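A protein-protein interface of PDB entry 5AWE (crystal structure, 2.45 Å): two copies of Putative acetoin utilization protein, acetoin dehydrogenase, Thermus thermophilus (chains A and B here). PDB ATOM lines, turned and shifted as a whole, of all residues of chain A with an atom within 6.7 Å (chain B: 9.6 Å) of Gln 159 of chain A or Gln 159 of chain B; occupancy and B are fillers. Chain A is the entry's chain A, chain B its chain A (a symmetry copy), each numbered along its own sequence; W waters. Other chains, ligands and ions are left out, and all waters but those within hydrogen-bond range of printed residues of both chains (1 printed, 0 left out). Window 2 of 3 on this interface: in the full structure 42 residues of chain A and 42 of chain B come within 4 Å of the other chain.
Water W1 lies within hydrogen-bond range of the backbone carbonyl oxygen (O) of Pro 151 of chain B and the backbone NH (N) of Ile 166 of chain A.
Leu 154 of chain A touches Ile 166 of chain B, and with the chains exchanged Ile 166 of chain A touches Leu 154 of chain B. Ala 155 of chain B touches its own counterpart, Ala 155 of chain A. Ala 155 of chain A touches Ala 158 of chain B, and with the chains exchanged Ala 158 of chain A touches Ala 155 of chain B. Ala 155 of chain A touches Gln 159 of chain B, and with the chains exchanged Gln 159 of chain A touches Ala 155 of chain B. Positions printed for both chains: 152, 154, 155, 156, 157, 158, 159, 160, 161, 162, 166 and 196.
Of chain B, only Ala 155 (3.8 Å) and Gln 159 (3.95 Å) come within 4 Å of Gln 159 of chain A. Gln 159 of chain B touches just these residues of chain A: Ala 155 and Gln 159. No residue of chain B comes within 4 Å of Ala 160 of chain A. Pro 162 of chain A touches one residue of chain B. Of the printed residues of chain B, Ile 166 of chain A touches Leu 154 (3.8 Å). Printed residues of chain A within 4 Å of Leu 154 of chain B: Ile 166 (3.8 Å). The nearest residue of chain B that does not touch Gln 159 of chain A is Gln 156 of chain B (6.2 Å). The nearest printed residue of chain A that does not touch Ile 166 of chain B is Ala 155 of chain A (5.7 Å).
The backbone carbonyl oxygen of Ala 155 of chain A is in hydrogen-bond range of the side-chain amide nitrogen of Gln 159 of chain A (3.3 Å). The backbone carbonyl oxygen (O) of Pro 162 of chain A lies within hydrogen-bond range of the guanidinium group (NE) of Arg 196 of chain A (3.2 Å). The backbone carbonyl oxygen of Ala 155 of chain B lies within hydrogen-bond range of the side-chain amide nitrogen of Gln 159 of chain B, at 3.3 Å.
Ile 166 of chain B touches Leu 154 of chain A (CB to CD1, 3.8 Å). Ala 155 of chain A touches Ala 155 of chain B. Ala 155 of chain A touches Ala 158 of chain B (CB to CB, 3.7 Å). Ala 155 of chain A touches Gln 159 of chain B (CB to CG, 3.8 Å). Ala 155 of chain B touches Ala 158 of chain A (CB to CB, 3.7 Å). Gln 159 of chain A touches Ala 155 of chain B (CG to CB, 3.8 Å). Gln 159 of chain B touches Gln 159 of chain A. Pro 162 of chain A touches Pro 151 of chain B (CG to O, 3.6 Å). Ile 166 of chain A touches Leu 154 of chain B (CB to CD1, 3.8 Å).
Of the 12 printed residues of chain A, 6 touch a printed residue of chain B. Hydrophobic or aromatic side chains of chain A that line the printed part of chain B: Leu 154, Ala 155, Ala 158, Pro 162 and Ile 166. Printed residues of chain B that touch a printed residue of chain A: Pro 151, Leu 154, Ala 155, Ala 158, Gln 159 and Ile 166. Hydrophobic or aromatic side chains of chain B within 4 Å of the printed part of chain A: Pro 151, Leu 154, Ala 155, Ala 158 and Ile 166. Among the printed residues, no Asp or Glu carboxylate lies within 4 Å of a Lys or Arg side-chain nitrogen of the other chain.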
ATOM      1  N   GLY A 152      -5.853   7.522 -12.649  1.00  0.00           N
ATOM      2  CA  GLY A 152      -4.760   7.649 -11.703  1.00  0.00           C
ATOM      3  C   GLY A 152      -4.495   6.452 -10.799  1.00  0.00           C
ATOM      4  O   GLY A 152      -3.514   6.455 -10.047  1.00  0.00           O
ATOM      5  N   LEU A 154      -3.472   3.245 -11.053  1.00  0.00           N
ATOM      6  CA  LEU A 154      -2.318   2.357 -11.140  1.00  0.00           C
ATOM      7  C   LEU A 154      -1.097   3.017 -10.489  1.00  0.00           C
ATOM      8  O   LEU A 154      -0.354   2.382  -9.733  1.00  0.00           O
ATOM      9  CB  LEU A 154      -2.026   2.012 -12.597  1.00  0.00           C
ATOM     10  CG  LEU A 154      -1.079   0.828 -12.817  1.00  0.00           C
ATOM     11  CD1 LEU A 154      -1.216   0.328 -14.250  1.00  0.00           C
ATOM     12  CD2 LEU A 154       0.348   1.235 -12.530  1.00  0.00           C
ATOM     13  N   ALA A 155      -0.907   4.299 -10.765  1.00  0.00           N
ATOM     14  CA  ALA A 155       0.127   5.055 -10.084  1.00  0.00           C
ATOM     15  C   ALA A 155      -0.016   4.908  -8.565  1.00  0.00           C
ATOM     16  O   ALA A 155       0.974   4.698  -7.851  1.00  0.00           O
ATOM     17  CB  ALA A 155       0.041   6.517 -10.483  1.00  0.00           C
ATOM     18  N   GLN A 156      -1.247   5.010  -8.072  1.00  0.00           N
ATOM     19  CA  GLN A 156      -1.490   4.954  -6.629  1.00  0.00           C
ATOM     20  C   GLN A 156      -1.222   3.553  -6.070  1.00  0.00           C
ATOM     21  O   GLN A 156      -0.603   3.414  -5.020  1.00  0.00           O
ATOM     22  CB  GLN A 156      -2.929   5.394  -6.319  1.00  0.00           C
ATOM     23  CG  GLN A 156      -3.394   5.140  -4.885  1.00  0.00           C
ATOM     24  CD  GLN A 156      -2.799   6.109  -3.881  1.00  0.00           C
ATOM     25  OE1 GLN A 156      -3.013   7.319  -3.967  1.00  0.00           O
ATOM     26  NE2 GLN A 156      -2.045   5.578  -2.916  1.00  0.00           N
ATOM     27  N   MET A 157      -1.667   2.520  -6.783  1.00  0.00           N
ATOM     28  CA  MET A 157      -1.383   1.141  -6.382  1.00  0.00           C
ATOM     29  C   MET A 157       0.118   0.872  -6.310  1.00  0.00           C
ATOM     30  O   MET A 157       0.574   0.132  -5.441  1.00  0.00           O
ATOM     31  CB  MET A 157      -2.016   0.149  -7.363  1.00  0.00           C
ATOM     32  CG  MET A 157      -1.725  -1.323  -7.039  1.00  0.00           C
ATOM     33  SD  MET A 157      -0.161  -1.980  -7.705  1.00  0.00           S
ATOM     34  CE  MET A 157      -0.390  -1.614  -9.417  1.00  0.00           C
ATOM     35  N   ALA A 158       0.876   1.474  -7.229  1.00  0.00           N
ATOM     36  CA  ALA A 158       2.306   1.191  -7.373  1.00  0.00           C
ATOM     37  C   ALA A 158       3.140   1.682  -6.199  1.00  0.00           C
ATOM     38  O   ALA A 158       4.233   1.172  -5.960  1.00  0.00           O
ATOM     39  CB  ALA A 158       2.837   1.802  -8.662  1.00  0.00           C
ATOM     40  N   GLN A 159       2.631   2.666  -5.464  1.00  0.00           N
ATOM     41  CA  GLN A 159       3.357   3.203  -4.315  1.00  0.00           C
ATOM     42  C   GLN A 159       3.459   2.216  -3.150  1.00  0.00           C
ATOM     43  O   GLN A 159       4.285   2.386  -2.257  1.00  0.00           O
ATOM     44  CB  GLN A 159       2.702   4.498  -3.841  1.00  0.00           C
ATOM     45  CG  GLN A 159       2.846   5.632  -4.837  1.00  0.00           C
ATOM     46  CD  GLN A 159       1.772   6.690  -4.678  1.00  0.00           C
ATOM     47  OE1 GLN A 159       1.312   6.962  -3.568  1.00  0.00           O
ATOM     48  NE2 GLN A 159       1.361   7.292  -5.793  1.00  0.00           N
ATOM     49  N   ALA A 160       2.630   1.182  -3.161  1.00  0.00           N
ATOM     50  CA  ALA A 160       2.666   0.193  -2.098  1.00  0.00           C
ATOM     51  C   ALA A 160       3.827  -0.800  -2.260  1.00  0.00           C
ATOM     52  O   ALA A 160       4.266  -1.408  -1.284  1.00  0.00           O
ATOM     53  CB  ALA A 160       1.331  -0.559  -2.042  1.00  0.00           C
ATOM     54  N   VAL A 161       4.327  -0.963  -3.481  1.00  0.00           N
ATOM     55  CA  VAL A 161       5.329  -1.987  -3.745  1.00  0.00           C
ATOM     56  C   VAL A 161       6.709  -1.755  -3.103  1.00  0.00           C
ATOM     57  O   VAL A 161       7.290  -2.686  -2.528  1.00  0.00           O
ATOM     58  CB  VAL A 161       5.535  -2.195  -5.266  1.00  0.00           C
ATOM     59  CG1 VAL A 161       6.580  -3.295  -5.505  1.00  0.00           C
ATOM     60  CG2 VAL A 161       4.217  -2.568  -5.927  1.00  0.00           C
ATOM     61  N   PRO A 162       7.260  -0.526  -3.195  1.00  0.00           N
ATOM     62  CA  PRO A 162       8.579  -0.293  -2.589  1.00  0.00           C
ATOM     63  C   PRO A 162       8.619  -0.805  -1.156  1.00  0.00           C
ATOM     64  O   PRO A 162       7.607  -0.784  -0.461  1.00  0.00           O
ATOM     65  CB  PRO A 162       8.759   1.226  -2.677  1.00  0.00           C
ATOM     66  CG  PRO A 162       7.911   1.629  -3.833  1.00  0.00           C
ATOM     67  CD  PRO A 162       6.702   0.712  -3.766  1.00  0.00           C
ATOM     68  N   ILE A 166       8.523  -3.598  -9.354  1.00  0.00           N
ATOM     69  CA  ILE A 166       7.597  -4.180 -10.316  1.00  0.00           C
ATOM     70  C   ILE A 166       8.360  -4.496 -11.598  1.00  0.00           C
ATOM     71  O   ILE A 166       9.114  -3.656 -12.111  1.00  0.00           O
ATOM     72  CB  ILE A 166       6.479  -3.198 -10.652  1.00  0.00           C
ATOM     73  CG1 ILE A 166       5.723  -2.836  -9.378  1.00  0.00           C
ATOM     74  CG2 ILE A 166       5.554  -3.796 -11.705  1.00  0.00           C
ATOM     75  CD1 ILE A 166       5.073  -1.465  -9.436  1.00  0.00           C
ATOM     76  N   ARG A 196       0.932  -4.320   2.271  1.00  0.00           N
ATOM     77  CA  ARG A 196       0.940  -2.909   1.912  1.00  0.00           C
ATOM     78  C   ARG A 196      -0.169  -2.541   0.933  1.00  0.00           C
ATOM     79  O   ARG A 196      -0.809  -1.501   1.078  1.00  0.00           O
ATOM     80  CB  ARG A 196       2.295  -2.532   1.315  1.00  0.00           C
ATOM     81  CG  ARG A 196       3.455  -2.684   2.279  1.00  0.00           C
ATOM     82  CD  ARG A 196       4.685  -1.981   1.752  1.00  0.00           C
ATOM     83  NE  ARG A 196       5.330  -2.737   0.685  1.00  0.00           N
ATOM     84  CZ  ARG A 196       6.329  -3.588   0.885  1.00  0.00           C
ATOM     85  NH1 ARG A 196       6.790  -3.785   2.111  1.00  0.00           N
ATOM     86  NH2 ARG A 196       6.858  -4.251  -0.133  1.00  0.00           N
ATOM     87  N   ILE B 147      13.156   4.407 -17.033  1.00  0.00           N
ATOM     88  CA  ILE B 147      12.972   5.047 -15.741  1.00  0.00           C
ATOM     89  C   ILE B 147      14.110   4.617 -14.835  1.00  0.00           C
ATOM     90  O   ILE B 147      14.715   3.560 -15.048  1.00  0.00           O
ATOM     91  CB  ILE B 147      11.635   4.626 -15.086  1.00  0.00           C
ATOM     92  CG1 ILE B 147      11.586   3.101 -14.938  1.00  0.00           C
ATOM     93  CG2 ILE B 147      10.464   5.135 -15.915  1.00  0.00           C
ATOM     94  CD1 ILE B 147      10.393   2.595 -14.139  1.00  0.00           C
ATOM     95  N   PRO B 151      13.123   1.598  -6.524  1.00  0.00           N
ATOM     96  CA  PRO B 151      11.763   1.169  -6.165  1.00  0.00           C
ATOM     97  C   PRO B 151      10.599   2.106  -6.497  1.00  0.00           C
ATOM     98  O   PRO B 151       9.573   1.659  -7.010  1.00  0.00           O
ATOM     99  CB  PRO B 151      11.866   0.868  -4.669  1.00  0.00           C
ATOM    100  CG  PRO B 151      13.305   0.475  -4.485  1.00  0.00           C
ATOM    101  CD  PRO B 151      14.079   1.363  -5.426  1.00  0.00           C
ATOM    102  N   GLY B 152      10.735   3.393  -6.215  1.00  0.00           N
ATOM    103  CA  GLY B 152       9.589   4.268  -6.382  1.00  0.00           C
ATOM    104  C   GLY B 152       9.357   4.834  -7.777  1.00  0.00           C
ATOM    105  O   GLY B 152       8.341   5.498  -8.010  1.00  0.00           O
ATOM    106  N   ALA B 153      10.280   4.580  -8.701  1.00  0.00           N
ATOM    107  CA  ALA B 153      10.269   5.258 -10.003  1.00  0.00           C
ATOM    108  C   ALA B 153       9.038   4.980 -10.868  1.00  0.00           C
ATOM    109  O   ALA B 153       8.529   5.880 -11.533  1.00  0.00           O
ATOM    110  CB  ALA B 153      11.542   4.910 -10.793  1.00  0.00           C
ATOM    111  N   LEU B 154       8.563   3.741 -10.871  1.00  0.00           N
ATOM    112  CA  LEU B 154       7.475   3.364 -11.767  1.00  0.00           C
ATOM    113  C   LEU B 154       6.182   4.073 -11.352  1.00  0.00           C
ATOM    114  O   LEU B 154       5.444   4.603 -12.191  1.00  0.00           O
ATOM    115  CB  LEU B 154       7.282   1.851 -11.756  1.00  0.00           C
ATOM    116  CG  LEU B 154       6.428   1.288 -12.896  1.00  0.00           C
ATOM    117  CD1 LEU B 154       6.671  -0.212 -13.020  1.00  0.00           C
ATOM    118  CD2 LEU B 154       4.964   1.570 -12.646  1.00  0.00           C
ATOM    119  N   ALA B 155       5.922   4.106 -10.053  1.00  0.00           N
ATOM    120  CA  ALA B 155       4.807   4.882  -9.543  1.00  0.00           C
ATOM    121  C   ALA B 155       4.881   6.326 -10.052  1.00  0.00           C
ATOM    122  O   ALA B 155       3.872   6.900 -10.482  1.00  0.00           O
ATOM    123  CB  ALA B 155       4.816   4.856  -8.025  1.00  0.00           C
ATOM    124  N   GLN B 156       6.076   6.908 -10.011  1.00  0.00           N
ATOM    125  CA  GLN B 156       6.248   8.307 -10.410  1.00  0.00           C
ATOM    126  C   GLN B 156       6.044   8.489 -11.917  1.00  0.00           C
ATOM    127  O   GLN B 156       5.383   9.431 -12.343  1.00  0.00           O
ATOM    128  CB  GLN B 156       7.637   8.809  -9.986  1.00  0.00           C
ATOM    129  CG  GLN B 156       8.044  10.165 -10.562  1.00  0.00           C
ATOM    130  CD  GLN B 156       7.335  11.333  -9.904  1.00  0.00           C
ATOM    131  OE1 GLN B 156       7.473  11.558  -8.700  1.00  0.00           O
ATOM    132  NE2 GLN B 156       6.570  12.089 -10.694  1.00  0.00           N
ATOM    133  N   MET B 157       6.592   7.577 -12.719  1.00  0.00           N
ATOM    134  CA  MET B 157       6.380   7.611 -14.167  1.00  0.00           C
ATOM    135  C   MET B 157       4.898   7.517 -14.521  1.00  0.00           C
ATOM    136  O   MET B 157       4.448   8.147 -15.475  1.00  0.00           O
ATOM    137  CB  MET B 157       7.126   6.462 -14.852  1.00  0.00           C
ATOM    138  CG  MET B 157       6.917   6.398 -16.371  1.00  0.00           C
ATOM    139  SD  MET B 157       5.435   5.490 -16.922  1.00  0.00           S
ATOM    140  CE  MET B 157       5.727   3.939 -16.134  1.00  0.00           C
ATOM    141  N   ALA B 158       4.149   6.723 -13.751  1.00  0.00           N
ATOM    142  CA  ALA B 158       2.751   6.421 -14.062  1.00  0.00           C
ATOM    143  C   ALA B 158       1.827   7.622 -13.920  1.00  0.00           C
ATOM    144  O   ALA B 158       0.760   7.657 -14.528  1.00  0.00           O
ATOM    145  CB  ALA B 158       2.248   5.288 -13.180  1.00  0.00           C
ATOM    146  N   GLN B 159       2.232   8.606 -13.123  1.00  0.00           N
ATOM    147  CA  GLN B 159       1.414   9.801 -12.924  1.00  0.00           C
ATOM    148  C   GLN B 159       1.318  10.681 -14.172  1.00  0.00           C
ATOM    149  O   GLN B 159       0.437  11.532 -14.270  1.00  0.00           O
ATOM    150  CB  GLN B 159       1.957  10.618 -11.754  1.00  0.00           C
ATOM    151  CG  GLN B 159       1.790   9.920 -10.418  1.00  0.00           C
ATOM    152  CD  GLN B 159       2.782  10.402  -9.378  1.00  0.00           C
ATOM    153  OE1 GLN B 159       3.166  11.573  -9.366  1.00  0.00           O
ATOM    154  NE2 GLN B 159       3.210   9.496  -8.500  1.00  0.00           N
ATOM    155  N   ALA B 160       2.213  10.474 -15.127  1.00  0.00           N
ATOM    156  CA  ALA B 160       2.187  11.260 -16.348  1.00  0.00           C
ATOM    157  C   ALA B 160       1.105  10.785 -17.329  1.00  0.00           C
ATOM    158  O   ALA B 160       0.656  11.552 -18.180  1.00  0.00           O
ATOM    159  CB  ALA B 160       3.565  11.218 -17.021  1.00  0.00           C
ATOM    160  N   VAL B 161       0.679   9.531 -17.212  1.00  0.00           N
ATOM    161  CA  VAL B 161      -0.238   8.959 -18.188  1.00  0.00           C
ATOM    162  C   VAL B 161      -1.662   9.547 -18.192  1.00  0.00           C
ATOM    163  O   VAL B 161      -2.209   9.839 -19.265  1.00  0.00           O
ATOM    164  CB  VAL B 161      -0.352   7.424 -18.024  1.00  0.00           C
ATOM    165  CG1 VAL B 161      -1.308   6.856 -19.084  1.00  0.00           C
ATOM    166  CG2 VAL B 161       1.020   6.780 -18.154  1.00  0.00           C
ATOM    167  N   PRO B 162      -2.287   9.720 -17.008  1.00  0.00           N
ATOM    168  CA  PRO B 162      -3.648  10.277 -17.001  1.00  0.00           C
ATOM    169  C   PRO B 162      -3.727  11.536 -17.852  1.00  0.00           C
ATOM    170  O   PRO B 162      -2.756  12.280 -17.951  1.00  0.00           O
ATOM    171  CB  PRO B 162      -3.922  10.549 -15.518  1.00  0.00           C
ATOM    172  CG  PRO B 162      -3.045   9.584 -14.800  1.00  0.00           C
ATOM    173  CD  PRO B 162      -1.783   9.506 -15.642  1.00  0.00           C
ATOM    174  N   PRO B 163      -4.894  11.811 -18.453  1.00  0.00           N
ATOM    175  CA  PRO B 163      -6.157  11.062 -18.409  1.00  0.00           C
ATOM    176  C   PRO B 163      -6.181   9.693 -19.098  1.00  0.00           C
ATOM    177  O   PRO B 163      -7.212   9.001 -19.062  1.00  0.00           O
ATOM    178  CB  PRO B 163      -7.159  12.025 -19.045  1.00  0.00           C
ATOM    179  CG  PRO B 163      -6.345  12.790 -20.024  1.00  0.00           C
ATOM    180  CD  PRO B 163      -4.951  12.913 -19.434  1.00  0.00           C
ATOM    181  N   ALA B 164      -5.071   9.301 -19.726  1.00  0.00           N
ATOM    182  CA  ALA B 164      -5.014   8.014 -20.423  1.00  0.00           C
ATOM    183  C   ALA B 164      -4.767   6.860 -19.450  1.00  0.00           C
ATOM    184  O   ALA B 164      -4.402   7.082 -18.292  1.00  0.00           O
ATOM    185  CB  ALA B 164      -3.922   8.037 -21.496  1.00  0.00           C
ATOM    186  N   ILE B 166      -3.027   2.930 -18.527  1.00  0.00           N
ATOM    187  CA  ILE B 166      -2.017   1.919 -18.804  1.00  0.00           C
ATOM    188  C   ILE B 166      -2.691   0.550 -18.833  1.00  0.00           C
ATOM    189  O   ILE B 166      -3.471   0.209 -17.932  1.00  0.00           O
ATOM    190  CB  ILE B 166      -0.950   1.905 -17.715  1.00  0.00           C
ATOM    191  CG1 ILE B 166      -0.286   3.276 -17.639  1.00  0.00           C
ATOM    192  CG2 ILE B 166       0.064   0.802 -17.986  1.00  0.00           C
ATOM    193  CD1 ILE B 166       0.274   3.596 -16.266  1.00  0.00           C
ATOM    194  N   ILE B 169       2.638  -3.254 -18.797  1.00  0.00           N
ATOM    195  CA  ILE B 169       4.034  -2.849 -18.731  1.00  0.00           C
ATOM    196  C   ILE B 169       4.900  -4.097 -18.786  1.00  0.00           C
ATOM    197  O   ILE B 169       4.639  -5.072 -18.066  1.00  0.00           O
ATOM    198  CB  ILE B 169       4.328  -2.078 -17.423  1.00  0.00           C
ATOM    199  CG1 ILE B 169       3.606  -0.729 -17.450  1.00  0.00           C
ATOM    200  CG2 ILE B 169       5.823  -1.861 -17.256  1.00  0.00           C
ATOM    201  CD1 ILE B 169       3.589  -0.015 -16.114  1.00  0.00           C
ATOM    202  N   MET B 183       5.565  -0.079 -22.651  1.00  0.00           N
ATOM    203  CA  MET B 183       4.323   0.271 -21.975  1.00  0.00           C
ATOM    204  C   MET B 183       3.272   0.530 -23.037  1.00  0.00           C
ATOM    205  O   MET B 183       3.532   1.219 -24.017  1.00  0.00           O
ATOM    206  CB  MET B 183       4.530   1.532 -21.112  1.00  0.00           C
ATOM    207  CG  MET B 183       3.364   1.886 -20.184  1.00  0.00           C
ATOM    208  SD  MET B 183       3.524   3.542 -19.429  1.00  0.00           S
ATOM    209  CE  MET B 183       2.936   3.229 -17.904  1.00  0.00           C
ATOM    210  N   GLY B 192      -0.994  12.672 -25.785  1.00  0.00           N
ATOM    211  CA  GLY B 192      -0.320  13.591 -24.890  1.00  0.00           C
ATOM    212  C   GLY B 192       0.696  12.932 -23.981  1.00  0.00           C
ATOM    213  O   GLY B 192       1.503  13.620 -23.358  1.00  0.00           O
ATOM    214  N   VAL B 193       0.676  11.603 -23.909  1.00  0.00           N
ATOM    215  CA  VAL B 193       1.492  10.888 -22.928  1.00  0.00           C
ATOM    216  C   VAL B 193       2.988  11.096 -23.081  1.00  0.00           C
ATOM    217  O   VAL B 193       3.662  11.403 -22.103  1.00  0.00           O
ATOM    218  CB  VAL B 193       1.247   9.369 -22.955  1.00  0.00           C
ATOM    219  CG1 VAL B 193       2.138   8.706 -21.930  1.00  0.00           C
ATOM    220  CG2 VAL B 193      -0.209   9.058 -22.670  1.00  0.00           C
ATOM    221  N   ARG B 196       3.989  14.504 -21.706  1.00  0.00           N
ATOM    222  CA  ARG B 196       3.906  14.499 -20.251  1.00  0.00           C
ATOM    223  C   ARG B 196       5.037  13.714 -19.597  1.00  0.00           C
ATOM    224  O   ARG B 196       5.600  14.150 -18.593  1.00  0.00           O
ATOM    225  CB  ARG B 196       2.562  13.923 -19.809  1.00  0.00           C
ATOM    226  CG  ARG B 196       1.366  14.743 -20.252  1.00  0.00           C
ATOM    227  CD  ARG B 196       0.121  14.324 -19.506  1.00  0.00           C
ATOM    228  NE  ARG B 196      -0.417  13.063 -20.008  1.00  0.00           N
ATOM    229  CZ  ARG B 196      -1.366  12.985 -20.931  1.00  0.00           C
ATOM    230  NH1 ARG B 196      -1.876  14.093 -21.448  1.00  0.00           N
ATOM    231  NH2 ARG B 196      -1.798  11.803 -21.348  1.00  0.00           N
ATOM    232  N   LEU B 197       5.373  12.560 -20.169  1.00  0.00           N
ATOM    233  CA  LEU B 197       6.408  11.708 -19.599  1.00  0.00           C
ATOM    234  C   LEU B 197       7.746  12.432 -19.471  1.00  0.00           C
ATOM    235  O   LEU B 197       8.347  12.464 -18.399  1.00  0.00           O
ATOM    236  CB  LEU B 197       6.590  10.448 -20.449  1.00  0.00           C
ATOM    237  CG  LEU B 197       5.572   9.320 -20.245  1.00  0.00           C
ATOM    238  CD1 LEU B 197       5.742   8.255 -21.316  1.00  0.00           C
ATOM    239  CD2 LEU B 197       5.757   8.717 -18.857  1.00  0.00           C
ATOM    240  N   ALA B 200       7.832  15.558 -17.598  1.00  0.00           N
ATOM    241  CA  ALA B 200       7.978  15.146 -16.207  1.00  0.00           C
ATOM    242  C   ALA B 200       9.364  14.555 -15.974  1.00  0.00           C
ATOM    243  O   ALA B 200       9.594  13.867 -14.979  1.00  0.00           O
ATOM    244  CB  ALA B 200       6.903  14.121 -15.848  1.00  0.00           C
ATOM    245  N   GLU B 202      10.985  12.189 -17.569  1.00  0.00           N
ATOM    246  CA  GLU B 202      11.203  10.783 -17.879  1.00  0.00           C
ATOM    247  C   GLU B 202      11.931  10.659 -19.221  1.00  0.00           C
ATOM    248  O   GLU B 202      11.865  11.563 -20.057  1.00  0.00           O
ATOM    249  CB  GLU B 202       9.863  10.046 -17.927  1.00  0.00           C
ATOM    250  CG  GLU B 202       9.904   8.650 -17.340  1.00  0.00           C
ATOM    251  CD  GLU B 202      10.117   8.653 -15.836  1.00  0.00           C
ATOM    252  OE1 GLU B 202      11.190   8.198 -15.387  1.00  0.00           O
ATOM    253  OE2 GLU B 202       9.212   9.109 -15.103  1.00  0.00           O
HETATM  254  O   HOH W   1       8.416  -0.943  -7.541  1.00  0.00           O
